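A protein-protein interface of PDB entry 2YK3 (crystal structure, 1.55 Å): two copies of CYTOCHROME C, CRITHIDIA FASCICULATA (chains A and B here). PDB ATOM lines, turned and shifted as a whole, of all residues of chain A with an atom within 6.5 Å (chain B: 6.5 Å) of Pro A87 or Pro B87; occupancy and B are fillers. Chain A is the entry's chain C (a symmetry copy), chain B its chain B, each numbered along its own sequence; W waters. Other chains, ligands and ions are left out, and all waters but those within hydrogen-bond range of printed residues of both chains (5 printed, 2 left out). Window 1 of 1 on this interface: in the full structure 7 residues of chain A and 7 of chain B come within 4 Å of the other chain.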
ATOM      1  N   LYS A  61      -1.075   9.004  10.265  1.00  0.00           N
ATOM      2  CA  LYS A  61      -1.588   9.953   9.270  1.00  0.00           C
ATOM      3  C   LYS A  61      -1.423   9.412   7.847  1.00  0.00           C
ATOM      4  O   LYS A  61      -2.308   9.528   7.022  1.00  0.00           O
ATOM      5  CB  LYS A  61      -0.931  11.314   9.373  1.00  0.00           C
ATOM      6  CG  LYS A  61      -1.654  12.269   8.433  1.00  0.00           C
ATOM      7  CD  LYS A  61      -1.220  13.713   8.605  1.00  0.00           C
ATOM      8  CE  LYS A  61      -2.233  14.514   9.403  1.00  0.00           C
ATOM      9  NZ  LYS A  61      -2.043  15.938   8.956  1.00  0.00           N
ATOM     10  N   ALA A  62      -0.294   8.745   7.569  1.00  0.00           N
ATOM     11  CA  ALA A  62      -0.054   8.151   6.263  1.00  0.00           C
ATOM     12  C   ALA A  62      -1.140   7.129   5.888  1.00  0.00           C
ATOM     13  O   ALA A  62      -1.698   7.205   4.816  1.00  0.00           O
ATOM     14  CB  ALA A  62       1.331   7.499   6.184  1.00  0.00           C
ATOM     15  N   ASN A  63      -1.462   6.200   6.782  1.00  0.00           N
ATOM     16  CA  ASN A  63      -2.492   5.213   6.431  1.00  0.00           C
ATOM     17  C   ASN A  63      -3.902   5.855   6.401  1.00  0.00           C
ATOM     18  O   ASN A  63      -4.719   5.502   5.558  1.00  0.00           O
ATOM     19  CB  ASN A  63      -2.355   4.042   7.408  1.00  0.00           C
ATOM     20  CG  ASN A  63      -2.916   2.712   6.904  1.00  0.00           C
ATOM     21  OD1 ASN A  63      -2.456   1.669   7.408  1.00  0.00           O
ATOM     22  ND2 ASN A  63      -3.844   2.719   5.948  1.00  0.00           N
ATOM     23  N   ALA A  64      -4.178   6.773   7.327  1.00  0.00           N
ATOM     24  CA  ALA A  64      -5.463   7.498   7.290  1.00  0.00           C
ATOM     25  C   ALA A  64      -5.687   8.234   5.973  1.00  0.00           C
ATOM     26  O   ALA A  64      -6.808   8.252   5.465  1.00  0.00           O
ATOM     27  CB  ALA A  64      -5.613   8.436   8.472  1.00  0.00           C
ATOM     28  N   GLU A  65      -4.621   8.829   5.406  1.00  0.00           N
ATOM     29  CA  GLU A  65      -4.707   9.664   4.198  1.00  0.00           C
ATOM     30  C   GLU A  65      -4.359   8.923   2.890  1.00  0.00           C
ATOM     31  O   GLU A  65      -4.413   9.530   1.798  1.00  0.00           O
ATOM     32  CB  GLU A  65      -3.761  10.883   4.316  1.00  0.00           C
ATOM     33  CG  GLU A  65      -4.200  12.103   5.188  1.00  0.00           C
ATOM     34  CD  GLU A  65      -3.095  13.168   5.454  1.00  0.00           C
ATOM     35  OE1 GLU A  65      -2.053  13.368   4.706  1.00  0.00           O
ATOM     36  OE2 GLU A  65      -3.311  13.888   6.453  1.00  0.00           O
ATOM     37  N   SER A  66      -3.994   7.639   2.995  1.00  0.00           N
ATOM     38  CA  SER A  66      -3.496   6.816   1.876  1.00  0.00           C
ATOM     39  C   SER A  66      -4.350   6.755   0.599  1.00  0.00           C
ATOM     40  O   SER A  66      -3.796   6.646  -0.521  1.00  0.00           O
ATOM     41  CB  SER A  66      -3.112   5.395   2.323  1.00  0.00           C
ATOM     42  OG  SER A  66      -4.157   4.681   2.993  1.00  0.00           O
ATOM     43  N   GLY A  67      -5.670   6.799   0.780  1.00  0.00           N
ATOM     44  CA  GLY A  67      -6.618   6.893  -0.352  1.00  0.00           C
ATOM     45  C   GLY A  67      -6.514   5.825  -1.423  1.00  0.00           C
ATOM     46  O   GLY A  67      -6.761   6.094  -2.597  1.00  0.00           O
ATOM     47  N   PRO A  82       5.936  -2.532   2.704  1.00  0.00           N
ATOM     48  CA  PRO A  82       4.974  -1.549   3.206  1.00  0.00           C
ATOM     49  C   PRO A  82       5.577  -0.153   3.321  1.00  0.00           C
ATOM     50  O   PRO A  82       4.895   0.822   2.971  1.00  0.00           O
ATOM     51  CB  PRO A  82       4.537  -2.144   4.558  1.00  0.00           C
ATOM     52  CG  PRO A  82       4.570  -3.608   4.257  1.00  0.00           C
ATOM     53  CD  PRO A  82       5.821  -3.803   3.474  1.00  0.00           C
ATOM     54  N   M3L A  83       6.827  -0.073   3.790  1.00  0.00           N
ATOM     55  CA  M3L A  83       7.505   1.241   4.004  1.00  0.00           C
ATOM     56  CB  M3L A  83       8.884   1.101   4.686  1.00  0.00           C
ATOM     57  CG  M3L A  83       9.650   2.421   4.940  1.00  0.00           C
ATOM     58  CD  M3L A  83      10.919   2.023   5.698  1.00  0.00           C
ATOM     59  CE  M3L A  83      11.889   3.155   6.034  1.00  0.00           C
ATOM     60  NZ  M3L A  83      13.086   2.649   6.761  1.00  0.00           N
ATOM     61  C   M3L A  83       7.656   1.967   2.687  1.00  0.00           C
ATOM     62  O   M3L A  83       7.531   3.207   2.665  1.00  0.00           O
ATOM     63  CM1 M3L A  83      12.740   1.511   7.646  1.00  0.00           C
ATOM     64  CM2 M3L A  83      14.100   2.150   5.820  1.00  0.00           C
ATOM     65  CM3 M3L A  83      13.668   3.737   7.556  1.00  0.00           C
ATOM     66  N   LYS A  84       7.964   1.243   1.605  1.00  0.00           N
ATOM     67  CA  LYS A  84       8.121   1.872   0.270  1.00  0.00           C
ATOM     68  C   LYS A  84       6.780   2.377  -0.297  1.00  0.00           C
ATOM     69  O   LYS A  84       6.682   3.479  -0.868  1.00  0.00           O
ATOM     70  CB  LYS A  84       8.852   0.943  -0.696  1.00  0.00           C
ATOM     71  CG  LYS A  84       9.121   1.515  -2.082  1.00  0.00           C
ATOM     72  CD  LYS A  84       9.795   0.463  -2.925  1.00  0.00           C
ATOM     73  CE  LYS A  84      10.242   1.105  -4.268  1.00  0.00           C
ATOM     74  NZ  LYS A  84      10.397   0.119  -5.363  1.00  0.00           N
ATOM     75  N   PHE A  85       5.753   1.569  -0.120  1.00  0.00           N
ATOM     76  CA  PHE A  85       4.419   1.856  -0.608  1.00  0.00           C
ATOM     77  C   PHE A  85       3.714   2.955   0.187  1.00  0.00           C
ATOM     78  O   PHE A  85       3.037   3.837  -0.399  1.00  0.00           O
ATOM     79  CB  PHE A  85       3.587   0.563  -0.554  1.00  0.00           C
ATOM     80  CG  PHE A  85       2.222   0.718  -1.138  1.00  0.00           C
ATOM     81  CD1 PHE A  85       1.163   1.166  -0.361  1.00  0.00           C
ATOM     82  CD2 PHE A  85       1.999   0.441  -2.479  1.00  0.00           C
ATOM     83  CE1 PHE A  85      -0.107   1.335  -0.907  1.00  0.00           C
ATOM     84  CE2 PHE A  85       0.730   0.584  -3.032  1.00  0.00           C
ATOM     85  CZ  PHE A  85      -0.328   1.030  -2.240  1.00  0.00           C
ATOM     86  N   MET A  86       3.897   2.922   1.504  1.00  0.00           N
ATOM     87  CA  MET A  86       3.231   3.825   2.433  1.00  0.00           C
ATOM     88  C   MET A  86       4.226   4.406   3.440  1.00  0.00           C
ATOM     89  O   MET A  86       4.145   4.120   4.666  1.00  0.00           O
ATOM     90  CB  MET A  86       2.085   3.126   3.142  1.00  0.00           C
ATOM     91  CG  MET A  86       1.218   4.059   3.958  1.00  0.00           C
ATOM     92  SD  MET A  86      -0.133   3.205   4.736  1.00  0.00           S
ATOM     93  CE  MET A  86      -1.082   2.590   3.334  1.00  0.00           C
ATOM     94  N   PRO A  87       5.160   5.255   2.942  1.00  0.00           N
ATOM     95  CA  PRO A  87       6.129   5.827   3.875  1.00  0.00           C
ATOM     96  C   PRO A  87       5.412   6.599   4.996  1.00  0.00           C
ATOM     97  O   PRO A  87       4.409   7.293   4.762  1.00  0.00           O
ATOM     98  CB  PRO A  87       6.924   6.832   3.001  1.00  0.00           C
ATOM     99  CG  PRO A  87       6.122   7.002   1.753  1.00  0.00           C
ATOM    100  CD  PRO A  87       5.358   5.746   1.560  1.00  0.00           C
ATOM    101  N   GLY A  88       5.873   6.437   6.227  1.00  0.00           N
ATOM    102  CA  GLY A  88       5.142   6.969   7.352  1.00  0.00           C
ATOM    103  C   GLY A  88       4.178   5.991   8.040  1.00  0.00           C
ATOM    104  O   GLY A  88       3.674   6.347   9.104  1.00  0.00           O
ATOM    105  N   THR A  89       3.948   4.798   7.480  1.00  0.00           N
ATOM    106  CA  THR A  89       3.117   3.790   8.186  1.00  0.00           C
ATOM    107  C   THR A  89       3.786   3.381   9.519  1.00  0.00           C
ATOM    108  O   THR A  89       5.033   3.373   9.616  1.00  0.00           O
ATOM    109  CB  THR A  89       2.889   2.598   7.318  1.00  0.00           C
ATOM    110  OG1 THR A  89       1.964   1.698   7.962  1.00  0.00           O
ATOM    111  CG2 THR A  89       4.187   1.824   6.972  1.00  0.00           C
ATOM    112  N   LYS B  61       7.553  11.591   9.290  1.00  0.00           N
ATOM    113  CA  LYS B  61       7.923  10.218   8.950  1.00  0.00           C
ATOM    114  C   LYS B  61       7.718   9.929   7.450  1.00  0.00           C
ATOM    115  O   LYS B  61       8.571   9.350   6.790  1.00  0.00           O
ATOM    116  CB  LYS B  61       7.122   9.233   9.830  1.00  0.00           C
ATOM    117  CG  LYS B  61       7.398   9.366  11.360  1.00  0.00           C
ATOM    118  CD  LYS B  61       6.528   8.422  12.201  1.00  0.00           C
ATOM    119  CE  LYS B  61       5.119   9.001  12.407  1.00  0.00           C
ATOM    120  NZ  LYS B  61       5.108  10.324  13.126  1.00  0.00           N
ATOM    121  N   ALA B  62       6.592  10.375   6.899  1.00  0.00           N
ATOM    122  CA  ALA B  62       6.264  10.135   5.501  1.00  0.00           C
ATOM    123  C   ALA B  62       7.360  10.721   4.602  1.00  0.00           C
ATOM    124  O   ALA B  62       7.884  10.007   3.741  1.00  0.00           O
ATOM    125  CB  ALA B  62       4.929  10.774   5.149  1.00  0.00           C
ATOM    126  N   ASN B  63       7.722  11.997   4.806  1.00  0.00           N
ATOM    127  CA  ASN B  63       8.700  12.641   3.904  1.00  0.00           C
ATOM    128  C   ASN B  63      10.086  12.096   4.137  1.00  0.00           C
ATOM    129  O   ASN B  63      10.854  11.960   3.195  1.00  0.00           O
ATOM    130  CB  ASN B  63       8.708  14.187   4.117  1.00  0.00           C
ATOM    131  CG  ASN B  63       9.177  15.007   2.907  1.00  0.00           C
ATOM    132  OD1 ASN B  63       8.741  16.161   2.770  1.00  0.00           O
ATOM    133  ND2 ASN B  63      10.072  14.484   2.103  1.00  0.00           N
ATOM    134  N   ALA B  64      10.407  11.776   5.396  1.00  0.00           N
ATOM    135  CA  ALA B  64      11.717  11.164   5.718  1.00  0.00           C
ATOM    136  C   ALA B  64      11.911   9.835   4.983  1.00  0.00           C
ATOM    137  O   ALA B  64      13.016   9.524   4.517  1.00  0.00           O
ATOM    138  CB  ALA B  64      11.870  10.956   7.207  1.00  0.00           C
ATOM    139  N   GLU B  65      10.835   9.043   4.915  1.00  0.00           N
ATOM    140  CA  GLU B  65      10.883   7.684   4.377  1.00  0.00           C
ATOM    141  C   GLU B  65      10.522   7.597   2.889  1.00  0.00           C
ATOM    142  O   GLU B  65      10.579   6.484   2.323  1.00  0.00           O
ATOM    143  CB  GLU B  65       9.901   6.768   5.157  1.00  0.00           C
ATOM    144  CG  GLU B  65      10.302   6.398   6.613  1.00  0.00           C
ATOM    145  CD  GLU B  65       9.301   5.472   7.368  1.00  0.00           C
ATOM    146  OE1 GLU B  65       8.262   4.914   6.817  1.00  0.00           O
ATOM    147  OE2 GLU B  65       9.605   5.275   8.571  1.00  0.00           O
ATOM    148  N   SER B  66      10.159   8.729   2.264  1.00  0.00           N
ATOM    149  CA  SER B  66       9.473   8.784   0.949  1.00  0.00           C
ATOM    150  C   SER B  66      10.216   8.204  -0.263  1.00  0.00           C
ATOM    151  O   SER B  66       9.576   7.784  -1.242  1.00  0.00           O
ATOM    152  CB  SER B  66       8.968  10.194   0.619  1.00  0.00           C
ATOM    153  OG  SER B  66      10.030  11.141   0.579  1.00  0.00           O
ATOM    154  N   GLY B  67      11.546   8.230  -0.202  1.00  0.00           N
ATOM    155  CA  GLY B  67      12.386   7.546  -1.210  1.00  0.00           C
ATOM    156  C   GLY B  67      12.143   7.893  -2.666  1.00  0.00           C
ATOM    157  O   GLY B  67      12.290   7.062  -3.542  1.00  0.00           O
ATOM    158  N   PRO B  82      -0.137  17.421  -2.855  1.00  0.00           N
ATOM    159  CA  PRO B  82       0.874  16.842  -1.980  1.00  0.00           C
ATOM    160  C   PRO B  82       0.336  15.721  -1.089  1.00  0.00           C
ATOM    161  O   PRO B  82       0.992  14.676  -0.936  1.00  0.00           O
ATOM    162  CB  PRO B  82       1.325  18.054  -1.154  1.00  0.00           C
ATOM    163  CG  PRO B  82       1.252  19.171  -2.141  1.00  0.00           C
ATOM    164  CD  PRO B  82      -0.093  18.895  -2.820  1.00  0.00           C
ATOM    165  N   M3L B  83      -0.863  15.910  -0.566  1.00  0.00           N
ATOM    166  CA  M3L B  83      -1.484  14.888   0.299  1.00  0.00           C
ATOM    167  CB  M3L B  83      -2.813  15.428   0.830  1.00  0.00           C
ATOM    168  CG  M3L B  83      -3.519  14.525   1.837  1.00  0.00           C
ATOM    169  CD  M3L B  83      -4.843  15.170   2.191  1.00  0.00           C
ATOM    170  CE  M3L B  83      -4.774  16.038   3.436  1.00  0.00           C
ATOM    171  NZ  M3L B  83      -6.131  16.101   4.046  1.00  0.00           N
ATOM    172  C   M3L B  83      -1.665  13.582  -0.440  1.00  0.00           C
ATOM    173  O   M3L B  83      -1.527  12.499   0.188  1.00  0.00           O
ATOM    174  CM1 M3L B  83      -6.734  17.402   3.745  1.00  0.00           C
ATOM    175  CM2 M3L B  83      -7.015  15.025   3.563  1.00  0.00           C
ATOM    176  CM3 M3L B  83      -6.070  15.894   5.495  1.00  0.00           C
ATOM    177  N   LYS B  84      -2.093  13.646  -1.702  1.00  0.00           N
ATOM    178  CA  LYS B  84      -2.363  12.430  -2.463  1.00  0.00           C
ATOM    179  C   LYS B  84      -1.061  11.711  -2.774  1.00  0.00           C
ATOM    180  O   LYS B  84      -0.967  10.467  -2.662  1.00  0.00           O
ATOM    181  CB  LYS B  84      -3.165  12.739  -3.727  1.00  0.00           C
ATOM    182  CG  LYS B  84      -3.492  11.517  -4.553  1.00  0.00           C
ATOM    183  CD  LYS B  84      -4.399  11.823  -5.736  1.00  0.00           C
ATOM    184  CE  LYS B  84      -4.931  10.521  -6.322  1.00  0.00           C
ATOM    185  NZ  LYS B  84      -6.217  10.672  -7.092  1.00  0.00           N
ATOM    186  N   PHE B  85      -0.026  12.477  -3.116  1.00  0.00           N
ATOM    187  CA  PHE B  85       1.241  11.887  -3.475  1.00  0.00           C
ATOM    188  C   PHE B  85       1.995  11.341  -2.269  1.00  0.00           C
ATOM    189  O   PHE B  85       2.633  10.299  -2.356  1.00  0.00           O
ATOM    190  CB  PHE B  85       2.096  12.944  -4.196  1.00  0.00           C
ATOM    191  CG  PHE B  85       3.454  12.451  -4.601  1.00  0.00           C
ATOM    192  CD1 PHE B  85       3.646  11.823  -5.841  1.00  0.00           C
ATOM    193  CD2 PHE B  85       4.526  12.583  -3.753  1.00  0.00           C
ATOM    194  CE1 PHE B  85       4.919  11.331  -6.214  1.00  0.00           C
ATOM    195  CE2 PHE B  85       5.819  12.091  -4.122  1.00  0.00           C
ATOM    196  CZ  PHE B  85       6.002  11.485  -5.349  1.00  0.00           C
ATOM    197  N   MET B  86       1.941  12.079  -1.168  1.00  0.00           N
ATOM    198  CA  MET B  86       2.690  11.760   0.057  1.00  0.00           C
ATOM    199  C   MET B  86       1.783  11.834   1.278  1.00  0.00           C
ATOM    200  O   MET B  86       1.934  12.744   2.125  1.00  0.00           O
ATOM    201  CB  MET B  86       3.870  12.720   0.241  1.00  0.00           C
ATOM    202  CG  MET B  86       4.861  12.253   1.260  1.00  0.00           C
ATOM    203  SD  MET B  86       6.163  13.467   1.568  1.00  0.00           S
ATOM    204  CE  MET B  86       6.994  13.561  -0.038  1.00  0.00           C
ATOM    205  N   PRO B  87       0.851  10.873   1.416  1.00  0.00           N
ATOM    206  CA  PRO B  87      -0.047  10.938   2.561  1.00  0.00           C
ATOM    207  C   PRO B  87       0.754  10.892   3.885  1.00  0.00           C
ATOM    208  O   PRO B  87       1.727  10.122   4.017  1.00  0.00           O
ATOM    209  CB  PRO B  87      -0.930   9.693   2.404  1.00  0.00           C
ATOM    210  CG  PRO B  87      -0.260   8.860   1.420  1.00  0.00           C
ATOM    211  CD  PRO B  87       0.536   9.736   0.535  1.00  0.00           C
ATOM    212  N   GLY B  88       0.358  11.715   4.842  1.00  0.00           N
ATOM    213  CA  GLY B  88       1.150  11.847   6.055  1.00  0.00           C
ATOM    214  C   GLY B  88       2.160  13.002   6.036  1.00  0.00           C
ATOM    215  O   GLY B  88       2.793  13.262   7.049  1.00  0.00           O
ATOM    216  N   THR B  89       2.339  13.677   4.898  1.00  0.00           N
ATOM    217  CA  THR B  89       3.184  14.882   4.901  1.00  0.00           C
ATOM    218  C   THR B  89       2.617  15.975   5.841  1.00  0.00           C
ATOM    219  O   THR B  89       1.384  16.053   6.049  1.00  0.00           O
ATOM    220  CB  THR B  89       3.389  15.382   3.486  1.00  0.00           C
ATOM    221  OG1 THR B  89       4.302  16.497   3.501  1.00  0.00           O
ATOM    222  CG2 THR B  89       2.070  15.814   2.884  1.00  0.00           C
HETATM  223  O   HOH W   1       3.001   8.138   2.614  1.00  0.00           O
HETATM  224  O   HOH W   2      -1.057  15.878   4.581  1.00  0.00           O
HETATM  225  O   HOH W   3       7.298   2.666   8.089  1.00  0.00           O
HETATM  226  O   HOH W   4      -2.900   8.475  -2.114  1.00  0.00           O
HETATM  227  O   HOH W   5       8.245   5.494  -1.510  1.00  0.00           O
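Of chain B, only Ala B62 (3.4 Å), Glu B65 (3.7 Å), Ser B66 (3.8 Å) and Pro B87 (3.97 Å) come within 4 Å of Pro A87.
Pro B87 touches just these residues of chain A: Ala A62 (3.4 Å), Glu A65 (3.5 Å), Ser A66 (3.7 Å) and Pro A87 (3.97 Å).
Of the printed residues of chain A, Lys B61 touches Gly A88.
Printed residues of chain A within 4 Å of Ser B66: Pro A87 (3.8 Å).
Of the printed residues of chain A, Ala B62 touches Pro A87 and Gly A88.
Ala A64 touches none of the printed residues of chain B.
Met B86 touches none of the printed residues of chain A.
The nearest residue of chain B that does not touch Pro A87 is Lys B61 (4.6 Å).
The nearest residue of chain A that does not touch Pro B87 is Lys A61 (4.6 Å).
The nearest printed residue of chain A that does not touch Gly B88 is Pro A87 (5.7 Å).
Lys A61 touches Gly B88, and with the chains exchanged Gly A88 touches Lys B61.
Ala A62 touches Pro B87, and with the chains exchanged Pro A87 touches Ala B62.
Glu A65 touches M3L B83, and with the chains exchanged M3L A83 touches Glu B65.
Pro B87 touches its own counterpart, Pro A87.
Of the 15 pairs that touch across the chains among the printed residues, 15 have their exchanged pair printed and touching as well.
Among the printed residues, merely in contact across the chains: Lys A61 with Gly B88 (3.7 Å), Ala A62 with Pro B87 (3.4 Å), Ala A62 with Gly B88 (3.7 Å), Glu A65 with M3L B83 (3.4 Å), Glu A65 with Pro B87 (3.5 Å), Ser A66 with Pro B87 (3.7 Å), M3L A83 with Glu B65 (3.4 Å), Pro A87 with Ala B62 (3.4 Å), Pro A87 with Glu B65 (3.7 Å), Pro A87 with Ser B66 (3.8 Å), Pro A87 with Pro B87 (3.97 Å), Gly A88 with Lys B61 (3.9 Å) and Gly A88 with Ala B62 (3.7 Å).
Printed residues of chain A that touch a printed residue of chain B: Lys A61, Ala A62, Glu A65, Ser A66, M3L A83, Pro A87 and Gly A88.
Along chain A the printed residues that touch a printed residue of chain B span positions 61 to 88.
Among the printed residues, 15 pairs touch across the chains.
Water W4 lies within hydrogen-bond range of the backbone carbonyl oxygen of Ser A66 and the backbone carbonyl oxygen of Lys B84.
Water W5 lies within hydrogen-bond range of O of Lys A84 (2.6 Å) and O of Ser B66 (2.7 Å).
Water W2 bridges the side-chain carboxylate of Glu A65 and the backbone carbonyl oxygen of Thr B89.
Water W1 bridges O of Pro A87 (2.7 Å) and O of Pro B87 (2.7 Å).
Water W3 bridges the side-chain carboxylate of Glu B65 (2.8 Å) and the backbone carbonyl oxygen of Thr A89 (2.8 Å).
The side-chain carboxylate (OE2) of Glu A65 lies within salt-bridge range of the side-chain amino group (NZ) of Lys A61 (3.5 Å).
The backbone carbonyl oxygen (O) of Asn A63 is in hydrogen-bond range of the side-chain hydroxyl (OG) of Ser A66.
O of Asn B63 is in hydrogen-bond range of OG of Ser B66 (2.9 Å).
The backbone NH (N) of Gly A88 lies within hydrogen-bond range of the side-chain carboxylate (OE1) of Glu B65, at 2.9 Å.
The backbone NH (N) of Gly B88 is in hydrogen-bond range of the side-chain carboxylate (OE1) of Glu A65 (2.9 Å).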
